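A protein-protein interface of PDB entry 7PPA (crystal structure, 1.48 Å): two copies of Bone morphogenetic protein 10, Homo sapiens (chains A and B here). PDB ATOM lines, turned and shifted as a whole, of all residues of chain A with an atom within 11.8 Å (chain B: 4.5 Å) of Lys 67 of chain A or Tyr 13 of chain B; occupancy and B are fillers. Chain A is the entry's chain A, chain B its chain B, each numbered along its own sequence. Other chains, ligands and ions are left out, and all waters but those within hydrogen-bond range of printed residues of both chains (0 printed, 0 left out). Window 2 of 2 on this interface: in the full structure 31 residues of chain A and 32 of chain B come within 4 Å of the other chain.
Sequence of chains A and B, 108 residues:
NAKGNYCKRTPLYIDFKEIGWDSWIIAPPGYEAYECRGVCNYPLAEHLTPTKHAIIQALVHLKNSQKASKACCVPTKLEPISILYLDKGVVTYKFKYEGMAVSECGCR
No position is printed for both chains.
Of the 9 printed residues of chain B, 5 touch a printed residue of chain A.
Along chain B the printed residues that touch a printed residue of chain A span positions 12 to 35.
Printed residues of chain A that touch a printed residue of chain B: Ile 56, Gln 57, Val 60, Lys 67, Ala 68 and Ser 69.
Hydrophobic or aromatic side chains of chain A that line the printed part of chain B: Ile 56, Val 60 and Ala 68.
Among the printed residues, 9 pairs touch across the chains.
A ring nitrogen (ND1) of His 61 of chain A is in hydrogen-bond range of the backbone carbonyl oxygen of Ala 68 of chain A (2.7 Å).
The backbone NH of Lys 67 of chain A lies within hydrogen-bond range of the side-chain amide oxygen of Asn 64 of chain A (3.4 Å).
The backbone NH (N) of Leu 12 of chain B is in hydrogen-bond range of the side-chain carboxylate (OE2) of Glu 32 of chain B, at 2.8 Å.
The backbone carbonyl oxygen (O) of Lys 70 of chain A is in hydrogen-bond range of the side-chain amide nitrogen (NE2) of Gln 57 of chain A, 3.3 Å away.
The backbone carbonyl oxygen of Tyr 31 of chain B sits at hydrogen-bond distance from the backbone NH of Ile 14 of chain B, 2.8 Å away.
The backbone carbonyl oxygen (O) of Ser 69 of chain A is in hydrogen-bond range of the side-chain amide nitrogen (NE2) of Gln 57 of chain A, at 2.9 Å.
The side-chain hydroxyl of Ser 69 of chain A lies within hydrogen-bond range of the side-chain carboxylate of Glu 35 of chain B, at 3.2 Å.
The backbone carbonyl oxygen of Tyr 13 of chain B lies within hydrogen-bond range of the side-chain amino group of Lys 67 of chain A, at 2.7 Å.
Among the printed residues, pairs that only touch across the chains: Ile 56 of chain A with Tyr 31 of chain B, Val 60 of chain A with Ile 14 of chain B, Ile 56 of chain A with Ile 14 of chain B, Lys 67 of chain A with Leu 12 of chain B, Ala 68 of chain A with Glu 35 of chain B, Lys 67 of chain A with Glu 35 of chain B and Gln 57 of chain A with Glu 35 of chain B.
Printed residues of chain B within 4 Å of Ile 56 of chain A: Ile 14 (3.6 Å) and Tyr 31 (3.4 Å).
Printed residues of chain B within 4 Å of Val 60 of chain A: Ile 14 (3.6 Å).
Gln 66 of chain A touches none of the printed residues of chain B.
Printed residues of chain B within 4 Å of Lys 67 of chain A: Leu 12, Tyr 13 and Glu 35.
Of the printed residues of chain B, Ala 68 of chain A touches Glu 35 (3.7 Å).
Printed residues of chain B within 4 Å of Ser 69 of chain A: Glu 35.
Leu 12 of chain B touches just one residue of chain A: Lys 67 (3.6 Å).
Of chain A, only Lys 67 comes within 4 Å of Tyr 13 of chain B.
Of chain A, only Ile 56 and Val 60 come within 4 Å of Ile 14 of chain B.
No residue of chain A comes within 4 Å of Gly 30 of chain B.
Glu 32 of chain B touches none of the printed residues of chain A.
The nearest printed residue of chain B that does not touch Lys 67 of chain A is Asp 15 of chain B (4.7 Å).
The nearest printed residue of chain B that does not touch Ile 56 of chain A is Leu 12 of chain B (6.0 Å).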
ATOM      1  N   HIS A  53       5.660 -17.558 -19.158  1.00  0.00           N
ATOM      2  CA  HIS A  53       5.336 -18.246 -20.443  1.00  0.00           C
ATOM      3  C   HIS A  53       4.746 -19.628 -20.166  1.00  0.00           C
ATOM      4  O   HIS A  53       3.812 -20.028 -20.852  1.00  0.00           O
ATOM      5  CB  HIS A  53       6.546 -18.325 -21.358  1.00  0.00           C
ATOM      6  CG  HIS A  53       6.183 -18.818 -22.704  1.00  0.00           C
ATOM      7  ND1 HIS A  53       6.050 -20.169 -23.003  1.00  0.00           N
ATOM      8  CD2 HIS A  53       5.867 -18.152 -23.822  1.00  0.00           C
ATOM      9  CE1 HIS A  53       5.685 -20.280 -24.263  1.00  0.00           C
ATOM     10  NE2 HIS A  53       5.584 -19.058 -24.789  1.00  0.00           N
ATOM     11  N   ALA A  54       5.352 -20.404 -19.255  1.00  0.00           N
ATOM     12  CA  ALA A  54       4.887 -21.779 -18.983  1.00  0.00           C
ATOM     13  C   ALA A  54       3.459 -21.749 -18.424  1.00  0.00           C
ATOM     14  O   ALA A  54       2.609 -22.584 -18.839  1.00  0.00           O
ATOM     15  CB  ALA A  54       5.836 -22.500 -18.043  1.00  0.00           C
ATOM     16  N   ILE A  55       3.188 -20.805 -17.513  1.00  0.00           N
ATOM     17  CA  ILE A  55       1.858 -20.686 -16.896  1.00  0.00           C
ATOM     18  C   ILE A  55       0.852 -20.385 -18.003  1.00  0.00           C
ATOM     19  O   ILE A  55      -0.157 -21.056 -18.044  1.00  0.00           O
ATOM     20  CB  ILE A  55       1.871 -19.610 -15.820  1.00  0.00           C
ATOM     21  CG1 ILE A  55       2.756 -20.021 -14.657  1.00  0.00           C
ATOM     22  CG2 ILE A  55       0.439 -19.318 -15.373  1.00  0.00           C
ATOM     23  CD1 ILE A  55       2.998 -18.902 -13.709  1.00  0.00           C
ATOM     24  N   ILE A  56       1.179 -19.440 -18.882  1.00  0.00           N
ATOM     25  CA  ILE A  56       0.240 -19.017 -19.967  1.00  0.00           C
ATOM     26  C   ILE A  56       0.038 -20.188 -20.924  1.00  0.00           C
ATOM     27  O   ILE A  56      -1.096 -20.497 -21.270  1.00  0.00           O
ATOM     28  CB  ILE A  56       0.807 -17.794 -20.692  1.00  0.00           C
ATOM     29  CG1 ILE A  56       0.793 -16.615 -19.723  1.00  0.00           C
ATOM     30  CG2 ILE A  56      -0.008 -17.536 -21.941  1.00  0.00           C
ATOM     31  CD1 ILE A  56       1.462 -15.357 -20.207  1.00  0.00           C
ATOM     32  N   GLN A  57       1.117 -20.843 -21.329  1.00  0.00           N
ATOM     33  CA  GLN A  57       0.985 -21.956 -22.294  1.00  0.00           C
ATOM     34  C   GLN A  57       0.156 -23.094 -21.658  1.00  0.00           C
ATOM     35  O   GLN A  57      -0.622 -23.726 -22.356  1.00  0.00           O
ATOM     36  CB  GLN A  57       2.368 -22.435 -22.706  1.00  0.00           C
ATOM     37  CG  GLN A  57       2.304 -23.472 -23.816  1.00  0.00           C
ATOM     38  CD  GLN A  57       3.672 -24.015 -24.106  1.00  0.00           C
ATOM     39  OE1 GLN A  57       4.632 -23.253 -24.249  1.00  0.00           O
ATOM     40  NE2 GLN A  57       3.799 -25.336 -24.095  1.00  0.00           N
ATOM     41  N   ALA A  58       0.398 -23.403 -20.379  1.00  0.00           N
ATOM     42  CA  ALA A  58      -0.347 -24.440 -19.630  1.00  0.00           C
ATOM     43  C   ALA A  58      -1.845 -24.132 -19.626  1.00  0.00           C
ATOM     44  O   ALA A  58      -2.648 -25.051 -19.824  1.00  0.00           O
ATOM     45  CB  ALA A  58       0.210 -24.564 -18.224  1.00  0.00           C
ATOM     46  N   LEU A  59      -2.182 -22.882 -19.403  1.00  0.00           N
ATOM     47  CA  LEU A  59      -3.607 -22.442 -19.396  1.00  0.00           C
ATOM     48  C   LEU A  59      -4.193 -22.545 -20.796  1.00  0.00           C
ATOM     49  O   LEU A  59      -5.329 -23.025 -20.914  1.00  0.00           O
ATOM     50  CB  LEU A  59      -3.689 -21.010 -18.893  1.00  0.00           C
ATOM     51  CG  LEU A  59      -5.095 -20.481 -18.659  1.00  0.00           C
ATOM     52  CD1 LEU A  59      -5.980 -21.497 -17.922  1.00  0.00           C
ATOM     53  CD2 LEU A  59      -4.999 -19.189 -17.866  1.00  0.00           C
ATOM     54  N   VAL A  60      -3.457 -22.127 -21.828  1.00  0.00           N
ATOM     55  CA  VAL A  60      -3.967 -22.249 -23.225  1.00  0.00           C
ATOM     56  C   VAL A  60      -4.240 -23.726 -23.496  1.00  0.00           C
ATOM     57  O   VAL A  60      -5.248 -24.029 -24.085  1.00  0.00           O
ATOM     58  CB  VAL A  60      -3.013 -21.676 -24.290  1.00  0.00           C
ATOM     59  CG1 VAL A  60      -3.496 -21.997 -25.716  1.00  0.00           C
ATOM     60  CG2 VAL A  60      -2.863 -20.176 -24.111  1.00  0.00           C
ATOM     61  N   HIS A  61      -3.346 -24.622 -23.120  1.00  0.00           N
ATOM     62  CA  HIS A  61      -3.509 -26.077 -23.382  1.00  0.00           C
ATOM     63  C   HIS A  61      -4.786 -26.589 -22.691  1.00  0.00           C
ATOM     64  O   HIS A  61      -5.540 -27.370 -23.304  1.00  0.00           O
ATOM     65  CB  HIS A  61      -2.275 -26.870 -22.943  1.00  0.00           C
ATOM     66  CG  HIS A  61      -2.553 -28.333 -23.071  1.00  0.00           C
ATOM     67  ND1 HIS A  61      -2.422 -28.990 -24.270  1.00  0.00           N
ATOM     68  CD2 HIS A  61      -3.036 -29.237 -22.184  1.00  0.00           C
ATOM     69  CE1 HIS A  61      -2.773 -30.258 -24.117  1.00  0.00           C
ATOM     70  NE2 HIS A  61      -3.149 -30.435 -22.835  1.00  0.00           N
ATOM     71  N   LEU A  62      -5.007 -26.184 -21.440  1.00  0.00           N
ATOM     72  CA  LEU A  62      -6.215 -26.599 -20.691  1.00  0.00           C
ATOM     73  C   LEU A  62      -7.468 -26.113 -21.440  1.00  0.00           C
ATOM     74  O   LEU A  62      -8.423 -26.902 -21.589  1.00  0.00           O
ATOM     75  CB  LEU A  62      -6.132 -26.033 -19.275  1.00  0.00           C
ATOM     76  CG  LEU A  62      -7.283 -26.452 -18.361  1.00  0.00           C
ATOM     77  CD1 LEU A  62      -7.274 -27.970 -18.163  1.00  0.00           C
ATOM     78  CD2 LEU A  62      -7.201 -25.725 -17.021  1.00  0.00           C
ATOM     79  N   LYS A  63      -7.457 -24.881 -21.946  1.00  0.00           N
ATOM     80  CA  LYS A  63      -8.651 -24.321 -22.658  1.00  0.00           C
ATOM     81  C   LYS A  63      -8.827 -24.977 -24.027  1.00  0.00           C
ATOM     82  O   LYS A  63      -9.966 -25.242 -24.393  1.00  0.00           O
ATOM     83  CB  LYS A  63      -8.540 -22.804 -22.782  1.00  0.00           C
ATOM     84  CG  LYS A  63      -8.558 -22.076 -21.439  1.00  0.00           C
ATOM     85  CD  LYS A  63      -9.691 -22.544 -20.513  1.00  0.00           C
ATOM     86  CE  LYS A  63      -9.686 -21.894 -19.146  1.00  0.00           C
ATOM     87  NZ  LYS A  63     -10.349 -20.573 -19.181  1.00  0.00           N
ATOM     88  N   ASN A  64      -7.744 -25.217 -24.758  1.00  0.00           N
ATOM     89  CA  ASN A  64      -7.792 -25.694 -26.160  1.00  0.00           C
ATOM     90  C   ASN A  64      -6.533 -26.522 -26.424  1.00  0.00           C
ATOM     91  O   ASN A  64      -5.495 -25.928 -26.749  1.00  0.00           O
ATOM     92  CB  ASN A  64      -7.940 -24.519 -27.125  1.00  0.00           C
ATOM     93  CG  ASN A  64      -7.923 -24.946 -28.578  1.00  0.00           C
ATOM     94  OD1 ASN A  64      -7.789 -26.133 -28.901  1.00  0.00           O
ATOM     95  ND2 ASN A  64      -8.036 -23.972 -29.462  1.00  0.00           N
ATOM     96  N   SER A  65      -6.629 -27.840 -26.314  1.00  0.00           N
ATOM     97  CA  SER A  65      -5.439 -28.723 -26.370  1.00  0.00           C
ATOM     98  C   SER A  65      -4.806 -28.662 -27.761  1.00  0.00           C
ATOM     99  O   SER A  65      -3.617 -28.977 -27.883  1.00  0.00           O
ATOM    100  CB  SER A  65      -5.786 -30.123 -25.984  1.00  0.00           C
ATOM    101  OG  SER A  65      -6.855 -30.602 -26.782  1.00  0.00           O
ATOM    102  N   GLN A  66      -5.565 -28.271 -28.787  1.00  0.00           N
ATOM    103  CA  GLN A  66      -5.046 -28.218 -30.183  1.00  0.00           C
ATOM    104  C   GLN A  66      -4.234 -26.925 -30.369  1.00  0.00           C
ATOM    105  O   GLN A  66      -3.431 -26.872 -31.308  1.00  0.00           O
ATOM    106  CB  GLN A  66      -6.189 -28.346 -31.191  1.00  0.00           C
ATOM    107  CG  GLN A  66      -6.829 -29.737 -31.162  1.00  0.00           C
ATOM    108  CD  GLN A  66      -7.388 -30.205 -32.481  1.00  0.00           C
ATOM    109  OE1 GLN A  66      -7.135 -29.623 -33.534  1.00  0.00           O
ATOM    110  NE2 GLN A  66      -8.142 -31.292 -32.429  1.00  0.00           N
ATOM    111  N   LYS A  67      -4.416 -25.913 -29.519  1.00  0.00           N
ATOM    112  CA  LYS A  67      -3.727 -24.616 -29.724  1.00  0.00           C
ATOM    113  C   LYS A  67      -2.315 -24.634 -29.118  1.00  0.00           C
ATOM    114  O   LYS A  67      -1.397 -23.973 -29.680  1.00  0.00           O
ATOM    115  CB  LYS A  67      -4.540 -23.440 -29.178  1.00  0.00           C
ATOM    116  CG  LYS A  67      -3.928 -22.111 -29.590  1.00  0.00           C
ATOM    117  CD  LYS A  67      -4.685 -20.873 -29.231  1.00  0.00           C
ATOM    118  CE  LYS A  67      -4.001 -19.651 -29.805  1.00  0.00           C
ATOM    119  NZ  LYS A  67      -4.821 -18.434 -29.630  1.00  0.00           N
ATOM    120  N   ALA A  68      -2.105 -25.360 -28.028  1.00  0.00           N
ATOM    121  CA  ALA A  68      -0.765 -25.430 -27.396  1.00  0.00           C
ATOM    122  C   ALA A  68      -0.612 -26.751 -26.663  1.00  0.00           C
ATOM    123  O   ALA A  68      -1.617 -27.342 -26.222  1.00  0.00           O
ATOM    124  CB  ALA A  68      -0.532 -24.254 -26.463  1.00  0.00           C
ATOM    125  N   SER A  69       0.654 -27.141 -26.520  1.00  0.00           N
ATOM    126  CA  SER A  69       1.092 -28.347 -25.780  1.00  0.00           C
ATOM    127  C   SER A  69       1.214 -27.995 -24.294  1.00  0.00           C
ATOM    128  O   SER A  69       1.347 -26.800 -23.939  1.00  0.00           O
ATOM    129  CB  SER A  69       2.378 -28.868 -26.370  1.00  0.00           C
ATOM    130  OG  SER A  69       3.180 -27.765 -26.777  1.00  0.00           O
ATOM    131  N   LYS A  70       1.270 -29.018 -23.453  1.00  0.00           N
ATOM    132  CA  LYS A  70       1.615 -28.793 -22.040  1.00  0.00           C
ATOM    133  C   LYS A  70       3.026 -28.209 -21.928  1.00  0.00           C
ATOM    134  O   LYS A  70       3.872 -28.411 -22.810  1.00  0.00           O
ATOM    135  CB  LYS A  70       1.465 -30.091 -21.267  1.00  0.00           C
ATOM    136  CG  LYS A  70       0.020 -30.589 -21.178  1.00  0.00           C
ATOM    137  CD  LYS A  70      -0.133 -31.701 -20.143  1.00  0.00           C
ATOM    138  CE  LYS A  70      -1.226 -32.672 -20.522  1.00  0.00           C
ATOM    139  NZ  LYS A  70      -1.787 -33.307 -19.311  1.00  0.00           N
ATOM    140  N   ALA A  71       3.244 -27.485 -20.837  1.00  0.00           N
ATOM    141  CA  ALA A  71       4.583 -27.145 -20.337  1.00  0.00           C
ATOM    142  C   ALA A  71       5.308 -28.468 -20.069  1.00  0.00           C
ATOM    143  O   ALA A  71       4.687 -29.489 -19.867  1.00  0.00           O
ATOM    144  CB  ALA A  71       4.436 -26.299 -19.103  1.00  0.00           C
ATOM    145  N   PRO B  11       4.646 -20.719 -33.961  1.00  0.00           N
ATOM    146  CA  PRO B  11       3.700 -19.656 -33.600  1.00  0.00           C
ATOM    147  C   PRO B  11       2.793 -20.021 -32.418  1.00  0.00           C
ATOM    148  O   PRO B  11       2.416 -21.178 -32.314  1.00  0.00           O
ATOM    149  CB  PRO B  11       2.834 -19.448 -34.856  1.00  0.00           C
ATOM    150  CG  PRO B  11       3.167 -20.589 -35.816  1.00  0.00           C
ATOM    151  CD  PRO B  11       4.399 -21.298 -35.293  1.00  0.00           C
ATOM    152  N   LEU B  12       2.503 -19.058 -31.537  1.00  0.00           N
ATOM    153  CA  LEU B  12       1.454 -19.196 -30.493  1.00  0.00           C
ATOM    154  C   LEU B  12       0.982 -17.793 -30.136  1.00  0.00           C
ATOM    155  O   LEU B  12       1.746 -16.984 -29.572  1.00  0.00           O
ATOM    156  CB  LEU B  12       1.940 -19.926 -29.242  1.00  0.00           C
ATOM    157  CG  LEU B  12       0.915 -19.991 -28.100  1.00  0.00           C
ATOM    158  CD1 LEU B  12      -0.345 -20.757 -28.525  1.00  0.00           C
ATOM    159  CD2 LEU B  12       1.545 -20.651 -26.885  1.00  0.00           C
ATOM    160  N   TYR B  13      -0.237 -17.472 -30.576  1.00  0.00           N
ATOM    161  CA  TYR B  13      -0.828 -16.179 -30.186  1.00  0.00           C
ATOM    162  C   TYR B  13      -1.659 -16.370 -28.924  1.00  0.00           C
ATOM    163  O   TYR B  13      -2.478 -17.346 -28.851  1.00  0.00           O
ATOM    164  CB  TYR B  13      -1.673 -15.651 -31.337  1.00  0.00           C
ATOM    165  CG  TYR B  13      -2.178 -14.254 -31.038  1.00  0.00           C
ATOM    166  CD1 TYR B  13      -1.385 -13.139 -31.274  1.00  0.00           C
ATOM    167  CD2 TYR B  13      -3.364 -14.054 -30.355  1.00  0.00           C
ATOM    168  CE1 TYR B  13      -1.825 -11.843 -30.985  1.00  0.00           C
ATOM    169  CE2 TYR B  13      -3.788 -12.780 -30.005  1.00  0.00           C
ATOM    170  CZ  TYR B  13      -3.023 -11.665 -30.320  1.00  0.00           C
ATOM    171  OH  TYR B  13      -3.486 -10.428 -29.992  1.00  0.00           O
ATOM    172  N   ILE B  14      -1.445 -15.493 -27.959  1.00  0.00           N
ATOM    173  CA  ILE B  14      -2.214 -15.515 -26.690  1.00  0.00           C
ATOM    174  C   ILE B  14      -3.222 -14.393 -26.782  1.00  0.00           C
ATOM    175  O   ILE B  14      -2.776 -13.231 -26.797  1.00  0.00           O
ATOM    176  CB  ILE B  14      -1.354 -15.315 -25.440  1.00  0.00           C
ATOM    177  CG1 ILE B  14      -0.185 -16.305 -25.400  1.00  0.00           C
ATOM    178  CG2 ILE B  14      -2.265 -15.381 -24.210  1.00  0.00           C
ATOM    179  CD1 ILE B  14      -0.628 -17.737 -25.453  1.00  0.00           C
ATOM    180  N   ASP B  15      -4.500 -14.751 -26.767  1.00  0.00           N
ATOM    181  CA  ASP B  15      -5.591 -13.764 -26.623  1.00  0.00           C
ATOM    182  C   ASP B  15      -6.045 -13.832 -25.169  1.00  0.00           C
ATOM    183  O   ASP B  15      -6.498 -14.916 -24.717  1.00  0.00           O
ATOM    184  CB  ASP B  15      -6.675 -14.035 -27.661  1.00  0.00           C
ATOM    185  CG  ASP B  15      -7.827 -13.065 -27.560  1.00  0.00           C
ATOM    186  OD1 ASP B  15      -7.713 -11.925 -28.173  1.00  0.00           O
ATOM    187  OD2 ASP B  15      -8.804 -13.402 -26.830  1.00  0.00           O
ATOM    188  N   GLY B  30      -3.712  -9.100 -26.488  1.00  0.00           N
ATOM    189  CA  GLY B  30      -2.993 -10.384 -26.643  1.00  0.00           C
ATOM    190  C   GLY B  30      -1.636 -10.137 -27.225  1.00  0.00           C
ATOM    191  O   GLY B  30      -1.232  -8.969 -27.399  1.00  0.00           O
ATOM    192  N   TYR B  31      -0.857 -11.197 -27.433  1.00  0.00           N
ATOM    193  CA  TYR B  31       0.492 -10.987 -27.968  1.00  0.00           C
ATOM    194  C   TYR B  31       0.981 -12.316 -28.535  1.00  0.00           C
ATOM    195  O   TYR B  31       0.372 -13.385 -28.301  1.00  0.00           O
ATOM    196  CB  TYR B  31       1.380 -10.395 -26.868  1.00  0.00           C
ATOM    197  CG  TYR B  31       1.814 -11.428 -25.865  1.00  0.00           C
ATOM    198  CD1 TYR B  31       0.938 -11.915 -24.908  1.00  0.00           C
ATOM    199  CD2 TYR B  31       3.082 -11.953 -25.915  1.00  0.00           C
ATOM    200  CE1 TYR B  31       1.312 -12.896 -24.007  1.00  0.00           C
ATOM    201  CE2 TYR B  31       3.493 -12.910 -24.978  1.00  0.00           C
ATOM    202  CZ  TYR B  31       2.595 -13.400 -24.033  1.00  0.00           C
ATOM    203  OH  TYR B  31       2.939 -14.349 -23.110  1.00  0.00           O
ATOM    204  N   GLU B  32       2.034 -12.204 -29.322  1.00  0.00           N
ATOM    205  CA  GLU B  32       2.743 -13.381 -29.887  1.00  0.00           C
ATOM    206  C   GLU B  32       3.714 -13.931 -28.829  1.00  0.00           C
ATOM    207  O   GLU B  32       4.776 -13.346 -28.617  1.00  0.00           O
ATOM    208  CB  GLU B  32       3.474 -13.043 -31.186  1.00  0.00           C
ATOM    209  CG  GLU B  32       4.004 -14.270 -31.939  1.00  0.00           C
ATOM    210  CD  GLU B  32       2.970 -15.305 -32.372  1.00  0.00           C
ATOM    211  OE1 GLU B  32       1.822 -14.893 -32.630  1.00  0.00           O
ATOM    212  OE2 GLU B  32       3.304 -16.524 -32.438  1.00  0.00           O
ATOM    213  N   GLU B  35       5.908 -20.743 -29.108  1.00  0.00           N
ATOM    214  CA  GLU B  35       6.165 -21.942 -28.268  1.00  0.00           C
ATOM    215  C   GLU B  35       7.272 -22.748 -28.926  1.00  0.00           C
ATOM    216  O   GLU B  35       7.740 -22.364 -29.976  1.00  0.00           O
ATOM    217  CB  GLU B  35       4.908 -22.762 -27.969  1.00  0.00           C
ATOM    218  CG  GLU B  35       4.273 -23.343 -29.189  1.00  0.00           C
ATOM    219  CD  GLU B  35       3.069 -24.248 -28.935  1.00  0.00           C
ATOM    220  OE1 GLU B  35       2.879 -24.777 -27.798  1.00  0.00           O
ATOM    221  OE2 GLU B  35       2.308 -24.424 -29.903  1.00  0.00           O
